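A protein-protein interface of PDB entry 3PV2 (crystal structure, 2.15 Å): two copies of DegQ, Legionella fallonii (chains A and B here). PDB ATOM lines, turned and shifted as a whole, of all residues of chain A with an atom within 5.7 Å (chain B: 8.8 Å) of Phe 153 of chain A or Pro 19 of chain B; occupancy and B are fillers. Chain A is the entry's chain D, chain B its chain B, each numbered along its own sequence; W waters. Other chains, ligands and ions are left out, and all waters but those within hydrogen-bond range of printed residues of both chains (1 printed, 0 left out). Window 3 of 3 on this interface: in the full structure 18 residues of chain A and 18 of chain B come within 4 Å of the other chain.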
ATOM      1  N   GLY A 151     -10.973  17.420 -19.082  1.00  0.00           N
ATOM      2  CA  GLY A 151     -11.163  18.704 -18.401  1.00  0.00           C
ATOM      3  C   GLY A 151     -10.627  19.948 -19.069  1.00  0.00           C
ATOM      4  O   GLY A 151     -11.029  21.060 -18.698  1.00  0.00           O
ATOM      5  N   ASP A 152      -9.687  19.817 -20.006  1.00  0.00           N
ATOM      6  CA  ASP A 152      -9.138  20.992 -20.627  1.00  0.00           C
ATOM      7  C   ASP A 152     -10.236  21.623 -21.474  1.00  0.00           C
ATOM      8  O   ASP A 152     -11.036  20.911 -22.042  1.00  0.00           O
ATOM      9  CB  ASP A 152      -7.963  20.631 -21.539  1.00  0.00           C
ATOM     10  CG  ASP A 152      -6.661  20.284 -20.765  1.00  0.00           C
ATOM     11  OD1 ASP A 152      -6.553  20.675 -19.585  1.00  0.00           O
ATOM     12  OD2 ASP A 152      -5.723  19.659 -21.356  1.00  0.00           O
ATOM     13  N   PHE A 153     -10.252  22.949 -21.562  1.00  0.00           N
ATOM     14  CA  PHE A 153     -11.116  23.680 -22.468  1.00  0.00           C
ATOM     15  C   PHE A 153     -10.615  23.651 -23.893  1.00  0.00           C
ATOM     16  O   PHE A 153      -9.430  23.841 -24.165  1.00  0.00           O
ATOM     17  CB  PHE A 153     -11.363  25.134 -21.966  1.00  0.00           C
ATOM     18  CG  PHE A 153     -12.155  25.178 -20.666  1.00  0.00           C
ATOM     19  CD1 PHE A 153     -11.585  25.678 -19.508  1.00  0.00           C
ATOM     20  CD2 PHE A 153     -13.415  24.625 -20.600  1.00  0.00           C
ATOM     21  CE1 PHE A 153     -12.287  25.700 -18.328  1.00  0.00           C
ATOM     22  CE2 PHE A 153     -14.121  24.635 -19.426  1.00  0.00           C
ATOM     23  CZ  PHE A 153     -13.518  25.200 -18.275  1.00  0.00           C
ATOM     24  N   VAL A 154     -11.566  23.398 -24.796  1.00  0.00           N
ATOM     25  CA  VAL A 154     -11.317  23.368 -26.218  1.00  0.00           C
ATOM     26  C   VAL A 154     -12.407  24.085 -26.975  1.00  0.00           C
ATOM     27  O   VAL A 154     -13.579  24.157 -26.506  1.00  0.00           O
ATOM     28  CB  VAL A 154     -11.283  21.890 -26.706  1.00  0.00           C
ATOM     29  CG1 VAL A 154     -10.130  21.196 -26.155  1.00  0.00           C
ATOM     30  CG2 VAL A 154     -12.590  21.145 -26.266  1.00  0.00           C
ATOM     31  N   VAL A 155     -12.027  24.610 -28.151  1.00  0.00           N
ATOM     32  CA  VAL A 155     -12.929  25.139 -29.163  1.00  0.00           C
ATOM     33  C   VAL A 155     -12.740  24.393 -30.445  1.00  0.00           C
ATOM     34  O   VAL A 155     -11.629  24.192 -30.874  1.00  0.00           O
ATOM     35  CB  VAL A 155     -12.617  26.617 -29.407  1.00  0.00           C
ATOM     36  CG1 VAL A 155     -13.405  27.242 -30.578  1.00  0.00           C
ATOM     37  CG2 VAL A 155     -12.883  27.382 -28.137  1.00  0.00           C
ATOM     38  N   PHE A 174     -17.702  25.278 -28.148  1.00  0.00           N
ATOM     39  CA  PHE A 174     -16.927  25.296 -26.941  1.00  0.00           C
ATOM     40  C   PHE A 174     -17.239  24.082 -26.098  1.00  0.00           C
ATOM     41  O   PHE A 174     -18.357  23.705 -25.918  1.00  0.00           O
ATOM     42  CB  PHE A 174     -17.224  26.564 -26.146  1.00  0.00           C
ATOM     43  CG  PHE A 174     -16.462  26.680 -24.851  1.00  0.00           C
ATOM     44  CD1 PHE A 174     -15.140  27.144 -24.825  1.00  0.00           C
ATOM     45  CD2 PHE A 174     -17.079  26.429 -23.680  1.00  0.00           C
ATOM     46  CE1 PHE A 174     -14.472  27.249 -23.634  1.00  0.00           C
ATOM     47  CE2 PHE A 174     -16.422  26.527 -22.490  1.00  0.00           C
ATOM     48  CZ  PHE A 174     -15.119  26.928 -22.455  1.00  0.00           C
ATOM     49  N   GLY A 175     -16.206  23.507 -25.505  1.00  0.00           N
ATOM     50  CA  GLY A 175     -16.446  22.483 -24.490  1.00  0.00           C
ATOM     51  C   GLY A 175     -15.183  22.036 -23.819  1.00  0.00           C
ATOM     52  O   GLY A 175     -14.239  22.811 -23.719  1.00  0.00           O
ATOM     53  N   ILE A 176     -15.154  20.802 -23.353  1.00  0.00           N
ATOM     54  CA  ILE A 176     -13.939  20.265 -22.784  1.00  0.00           C
ATOM     55  C   ILE A 176     -13.506  18.994 -23.446  1.00  0.00           C
ATOM     56  O   ILE A 176     -14.255  18.417 -24.204  1.00  0.00           O
ATOM     57  CB  ILE A 176     -14.079  19.942 -21.271  1.00  0.00           C
ATOM     58  CG1 ILE A 176     -15.171  18.928 -21.014  1.00  0.00           C
ATOM     59  CG2 ILE A 176     -14.416  21.203 -20.524  1.00  0.00           C
ATOM     60  CD1 ILE A 176     -15.267  18.405 -19.518  1.00  0.00           C
ATOM     61  N   VAL A 177     -12.276  18.554 -23.147  1.00  0.00           N
ATOM     62  CA  VAL A 177     -11.843  17.242 -23.523  1.00  0.00           C
ATOM     63  C   VAL A 177     -12.584  16.320 -22.570  1.00  0.00           C
ATOM     64  O   VAL A 177     -12.455  16.458 -21.336  1.00  0.00           O
ATOM     65  CB  VAL A 177     -10.364  17.064 -23.332  1.00  0.00           C
ATOM     66  CG1 VAL A 177      -9.929  15.550 -23.545  1.00  0.00           C
ATOM     67  CG2 VAL A 177      -9.641  17.979 -24.199  1.00  0.00           C
ATOM     68  N   VAL A 210      -8.772  23.373 -30.993  1.00  0.00           N
ATOM     69  CA  VAL A 210      -7.730  24.158 -30.382  1.00  0.00           C
ATOM     70  C   VAL A 210      -7.899  24.185 -28.867  1.00  0.00           C
ATOM     71  O   VAL A 210      -9.013  24.113 -28.351  1.00  0.00           O
ATOM     72  CB  VAL A 210      -7.720  25.577 -30.934  1.00  0.00           C
ATOM     73  CG1 VAL A 210      -7.639  25.573 -32.462  1.00  0.00           C
ATOM     74  CG2 VAL A 210      -8.952  26.335 -30.464  1.00  0.00           C
ATOM     75  N   ASN A 211      -6.770  24.293 -28.150  1.00  0.00           N
ATOM     76  CA  ASN A 211      -6.815  24.431 -26.701  1.00  0.00           C
ATOM     77  C   ASN A 211      -7.103  25.894 -26.364  1.00  0.00           C
ATOM     78  O   ASN A 211      -7.281  26.711 -27.273  1.00  0.00           O
ATOM     79  CB  ASN A 211      -5.536  23.942 -26.039  1.00  0.00           C
ATOM     80  CG  ASN A 211      -4.320  24.691 -26.492  1.00  0.00           C
ATOM     81  OD1 ASN A 211      -4.403  25.802 -27.022  1.00  0.00           O
ATOM     82  ND2 ASN A 211      -3.173  24.104 -26.233  1.00  0.00           N
ATOM     83  N   ALA A 212      -7.192  26.180 -25.064  1.00  0.00           N
ATOM     84  CA  ALA A 212      -7.434  27.529 -24.549  1.00  0.00           C
ATOM     85  C   ALA A 212      -6.411  28.591 -24.948  1.00  0.00           C
ATOM     86  O   ALA A 212      -6.779  29.765 -24.997  1.00  0.00           O
ATOM     87  CB  ALA A 212      -7.595  27.517 -23.024  1.00  0.00           C
ATOM     88  N   PRO B  19      -7.095  28.718 -17.557  1.00  0.00           N
ATOM     89  CA  PRO B  19      -7.455  27.654 -16.639  1.00  0.00           C
ATOM     90  C   PRO B  19      -7.998  26.389 -17.321  1.00  0.00           C
ATOM     91  O   PRO B  19      -8.100  26.315 -18.541  1.00  0.00           O
ATOM     92  CB  PRO B  19      -8.579  28.292 -15.801  1.00  0.00           C
ATOM     93  CG  PRO B  19      -9.340  29.108 -16.845  1.00  0.00           C
ATOM     94  CD  PRO B  19      -8.252  29.589 -17.859  1.00  0.00           C
ATOM     95  N   SER B  20      -8.352  25.425 -16.480  1.00  0.00           N
ATOM     96  CA  SER B  20      -8.733  24.092 -16.902  1.00  0.00           C
ATOM     97  C   SER B  20      -9.479  23.468 -15.751  1.00  0.00           C
ATOM     98  O   SER B  20      -9.202  23.779 -14.589  1.00  0.00           O
ATOM     99  CB  SER B  20      -7.476  23.257 -17.149  1.00  0.00           C
ATOM    100  OG  SER B  20      -7.826  21.926 -17.426  1.00  0.00           O
ATOM    101  N   MET B  21     -10.368  22.534 -16.035  1.00  0.00           N
ATOM    102  CA  MET B  21     -10.944  21.758 -14.960  1.00  0.00           C
ATOM    103  C   MET B  21     -10.125  20.493 -14.698  1.00  0.00           C
ATOM    104  O   MET B  21     -10.408  19.769 -13.761  1.00  0.00           O
ATOM    105  CB  MET B  21     -12.392  21.403 -15.269  1.00  0.00           C
ATOM    106  CG  MET B  21     -13.387  22.533 -15.009  1.00  0.00           C
ATOM    107  SD  MET B  21     -13.824  22.695 -13.269  1.00  0.00           S
ATOM    108  CE  MET B  21     -14.163  21.022 -12.779  1.00  0.00           C
ATOM    109  N   ALA B  22      -9.120  20.227 -15.524  1.00  0.00           N
ATOM    110  CA  ALA B  22      -8.353  18.966 -15.443  1.00  0.00           C
ATOM    111  C   ALA B  22      -7.660  18.638 -14.109  1.00  0.00           C
ATOM    112  O   ALA B  22      -7.582  17.453 -13.762  1.00  0.00           O
ATOM    113  CB  ALA B  22      -7.323  18.900 -16.548  1.00  0.00           C
ATOM    114  N   PRO B  23      -7.155  19.644 -13.368  1.00  0.00           N
ATOM    115  CA  PRO B  23      -6.466  19.286 -12.105  1.00  0.00           C
ATOM    116  C   PRO B  23      -7.457  18.739 -11.031  1.00  0.00           C
ATOM    117  O   PRO B  23      -7.193  17.707 -10.387  1.00  0.00           O
ATOM    118  CB  PRO B  23      -5.802  20.611 -11.667  1.00  0.00           C
ATOM    119  CG  PRO B  23      -5.739  21.465 -12.865  1.00  0.00           C
ATOM    120  CD  PRO B  23      -6.973  21.067 -13.681  1.00  0.00           C
ATOM    121  N   PHE B 153     -21.052  26.441 -12.465  1.00  0.00           N
ATOM    122  CA  PHE B 153     -20.421  25.479 -13.358  1.00  0.00           C
ATOM    123  C   PHE B 153     -20.347  24.080 -12.779  1.00  0.00           C
ATOM    124  O   PHE B 153     -20.168  23.872 -11.585  1.00  0.00           O
ATOM    125  CB  PHE B 153     -19.055  25.986 -13.850  1.00  0.00           C
ATOM    126  CG  PHE B 153     -19.119  27.292 -14.651  1.00  0.00           C
ATOM    127  CD1 PHE B 153     -18.524  28.459 -14.163  1.00  0.00           C
ATOM    128  CD2 PHE B 153     -19.663  27.317 -15.917  1.00  0.00           C
ATOM    129  CE1 PHE B 153     -18.525  29.614 -14.911  1.00  0.00           C
ATOM    130  CE2 PHE B 153     -19.688  28.472 -16.629  1.00  0.00           C
ATOM    131  CZ  PHE B 153     -19.094  29.630 -16.113  1.00  0.00           C
ATOM    132  N   VAL B 154     -20.528  23.093 -13.630  1.00  0.00           N
ATOM    133  CA  VAL B 154     -20.513  21.726 -13.195  1.00  0.00           C
ATOM    134  C   VAL B 154     -19.867  20.830 -14.200  1.00  0.00           C
ATOM    135  O   VAL B 154     -19.821  21.133 -15.404  1.00  0.00           O
ATOM    136  CB  VAL B 154     -21.959  21.223 -12.935  1.00  0.00           C
ATOM    137  CG1 VAL B 154     -22.629  22.048 -11.788  1.00  0.00           C
ATOM    138  CG2 VAL B 154     -22.795  21.254 -14.223  1.00  0.00           C
ATOM    139  N   VAL B 155     -19.361  19.701 -13.701  1.00  0.00           N
ATOM    140  CA  VAL B 155     -18.879  18.632 -14.565  1.00  0.00           C
ATOM    141  C   VAL B 155     -19.579  17.338 -14.271  1.00  0.00           C
ATOM    142  O   VAL B 155     -19.758  16.974 -13.137  1.00  0.00           O
ATOM    143  CB  VAL B 155     -17.349  18.476 -14.449  1.00  0.00           C
ATOM    144  CG1 VAL B 155     -16.889  17.168 -15.168  1.00  0.00           C
ATOM    145  CG2 VAL B 155     -16.684  19.697 -15.041  1.00  0.00           C
ATOM    146  N   THR B 173     -18.181  15.742 -19.025  1.00  0.00           N
ATOM    147  CA  THR B 173     -18.843  16.775 -19.779  1.00  0.00           C
ATOM    148  C   THR B 173     -19.048  17.991 -18.870  1.00  0.00           C
ATOM    149  O   THR B 173     -19.104  17.859 -17.652  1.00  0.00           O
ATOM    150  CB  THR B 173     -20.195  16.266 -20.325  1.00  0.00           C
ATOM    151  OG1 THR B 173     -21.007  15.831 -19.218  1.00  0.00           O
ATOM    152  CG2 THR B 173     -19.968  15.070 -21.283  1.00  0.00           C
ATOM    153  N   PHE B 174     -19.116  19.143 -19.502  1.00  0.00           N
ATOM    154  CA  PHE B 174     -19.094  20.445 -18.889  1.00  0.00           C
ATOM    155  C   PHE B 174     -20.386  21.213 -19.203  1.00  0.00           C
ATOM    156  O   PHE B 174     -20.943  21.166 -20.338  1.00  0.00           O
ATOM    157  CB  PHE B 174     -17.910  21.247 -19.409  1.00  0.00           C
ATOM    158  CG  PHE B 174     -17.763  22.617 -18.764  1.00  0.00           C
ATOM    159  CD1 PHE B 174     -17.159  22.757 -17.502  1.00  0.00           C
ATOM    160  CD2 PHE B 174     -18.162  23.735 -19.413  1.00  0.00           C
ATOM    161  CE1 PHE B 174     -17.051  24.028 -16.896  1.00  0.00           C
ATOM    162  CE2 PHE B 174     -18.007  25.038 -18.852  1.00  0.00           C
ATOM    163  CZ  PHE B 174     -17.460  25.144 -17.560  1.00  0.00           C
ATOM    164  N   GLY B 175     -20.897  21.894 -18.175  1.00  0.00           N
ATOM    165  CA  GLY B 175     -21.952  22.868 -18.397  1.00  0.00           C
ATOM    166  C   GLY B 175     -22.255  23.619 -17.112  1.00  0.00           C
ATOM    167  O   GLY B 175     -21.375  23.750 -16.222  1.00  0.00           O
ATOM    168  N   ALA B 212     -17.300  23.193  -9.387  1.00  0.00           N
ATOM    169  CA  ALA B 212     -16.049  23.663  -9.902  1.00  0.00           C
ATOM    170  C   ALA B 212     -14.900  23.465  -8.942  1.00  0.00           C
ATOM    171  O   ALA B 212     -13.764  23.444  -9.372  1.00  0.00           O
ATOM    172  CB  ALA B 212     -16.173  25.174 -10.280  1.00  0.00           C
HETATM  173  O   HOH W   1      -8.058  24.535 -20.283  1.00  0.00           O
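Ser 20 of chain B touches Gly 151 of chain A (OG to O, 3.6 Å). O of Gly 151 of chain A touches N of Ala 22 of chain B, 3.8 Å away. Asp 152 of chain A touches Ala 22 of chain B. Phe 153 of chain A touches Pro 19 of chain B (CD1 to O, 3.7 Å). Phe 174 of chain B touches Phe 153 of chain A (CZ to CE2, 3.9 Å). Ile 176 of chain A touches Thr 173 of chain B. Phe 174 of chain B touches Ile 176 of chain A (CB to CG2, 3.7 Å).
No residue of chain B comes within 4 Å of Val 154 of chain A. Of the printed residues of chain B, Ile 176 of chain A touches Thr 173 (3.9 Å) and Phe 174 (3.7 Å). Of the printed residues of chain A, Pro 19 of chain B touches Phe 153. Printed residues of chain A within 4 Å of Ser 20 of chain B: Gly 151 (3.6 Å) and Asp 152 (2.8 Å). Of the printed residues of chain A, Met 21 of chain B touches Gly 151 (3.1 Å). The nearest residue of chain B that does not touch Phe 153 of chain A is Ser 20 of chain B (4.2 Å). The nearest residue of chain A that does not touch Pro 19 of chain B is Ala 212 of chain A (4.7 Å). The nearest printed residue of chain A that does not touch Met 21 of chain B is Phe 153 of chain A (4.2 Å).
OG of Ser 20 of chain B sits at hydrogen-bond distance from N of Ala 22 of chain B (2.9 Å). The backbone carbonyl oxygen (O) of Val 177 of chain A lies within hydrogen-bond range of the backbone NH (N) of Gly 151 of chain A. The backbone carbonyl oxygen of Asp 152 of chain A lies within hydrogen-bond range of the backbone NH of Val 177 of chain A (2.9 Å). The backbone carbonyl oxygen of Phe 153 of chain A lies within hydrogen-bond range of the backbone NH of Ala 212 of chain A (3.4 Å).
The side-chain carboxylate of Asp 152 of chain A is in hydrogen-bond range of the side-chain hydroxyl of Ser 20 of chain B, 2.8 Å away. The backbone carbonyl oxygen (O) of Gly 151 of chain A is in hydrogen-bond range of the backbone NH (N) of Met 21 of chain B, at 3.1 Å.
Phe 153 of chain A touches Phe 174 of chain B, but with the chains exchanged Phe 174 of chain A does not touch Phe 153 of chain B (7.0 Å). 6 positions are printed for both chains. Of the 9 pairs that touch across the chains among the printed residues, none has its exchanged pair printed and touching as well.
Of the 12 printed residues of chain A, 4 touch a printed residue of chain B. Printed residues of chain A that touch a printed residue of chain B: Gly 151, Asp 152, Phe 153 and Ile 176. Hydrophobic or aromatic side chains of chain B that line the printed part of chain A: Met 21, Ala 22 and Phe 174. Among the printed residues, no Asp or Glu carboxylate lies within 4 Å of a Lys or Arg side-chain nitrogen of the other chain.
Water W1 lies within hydrogen-bond range of O of Pro 19 of chain B (2.5 Å) and N of Phe 153 of chain A (3.0 Å).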
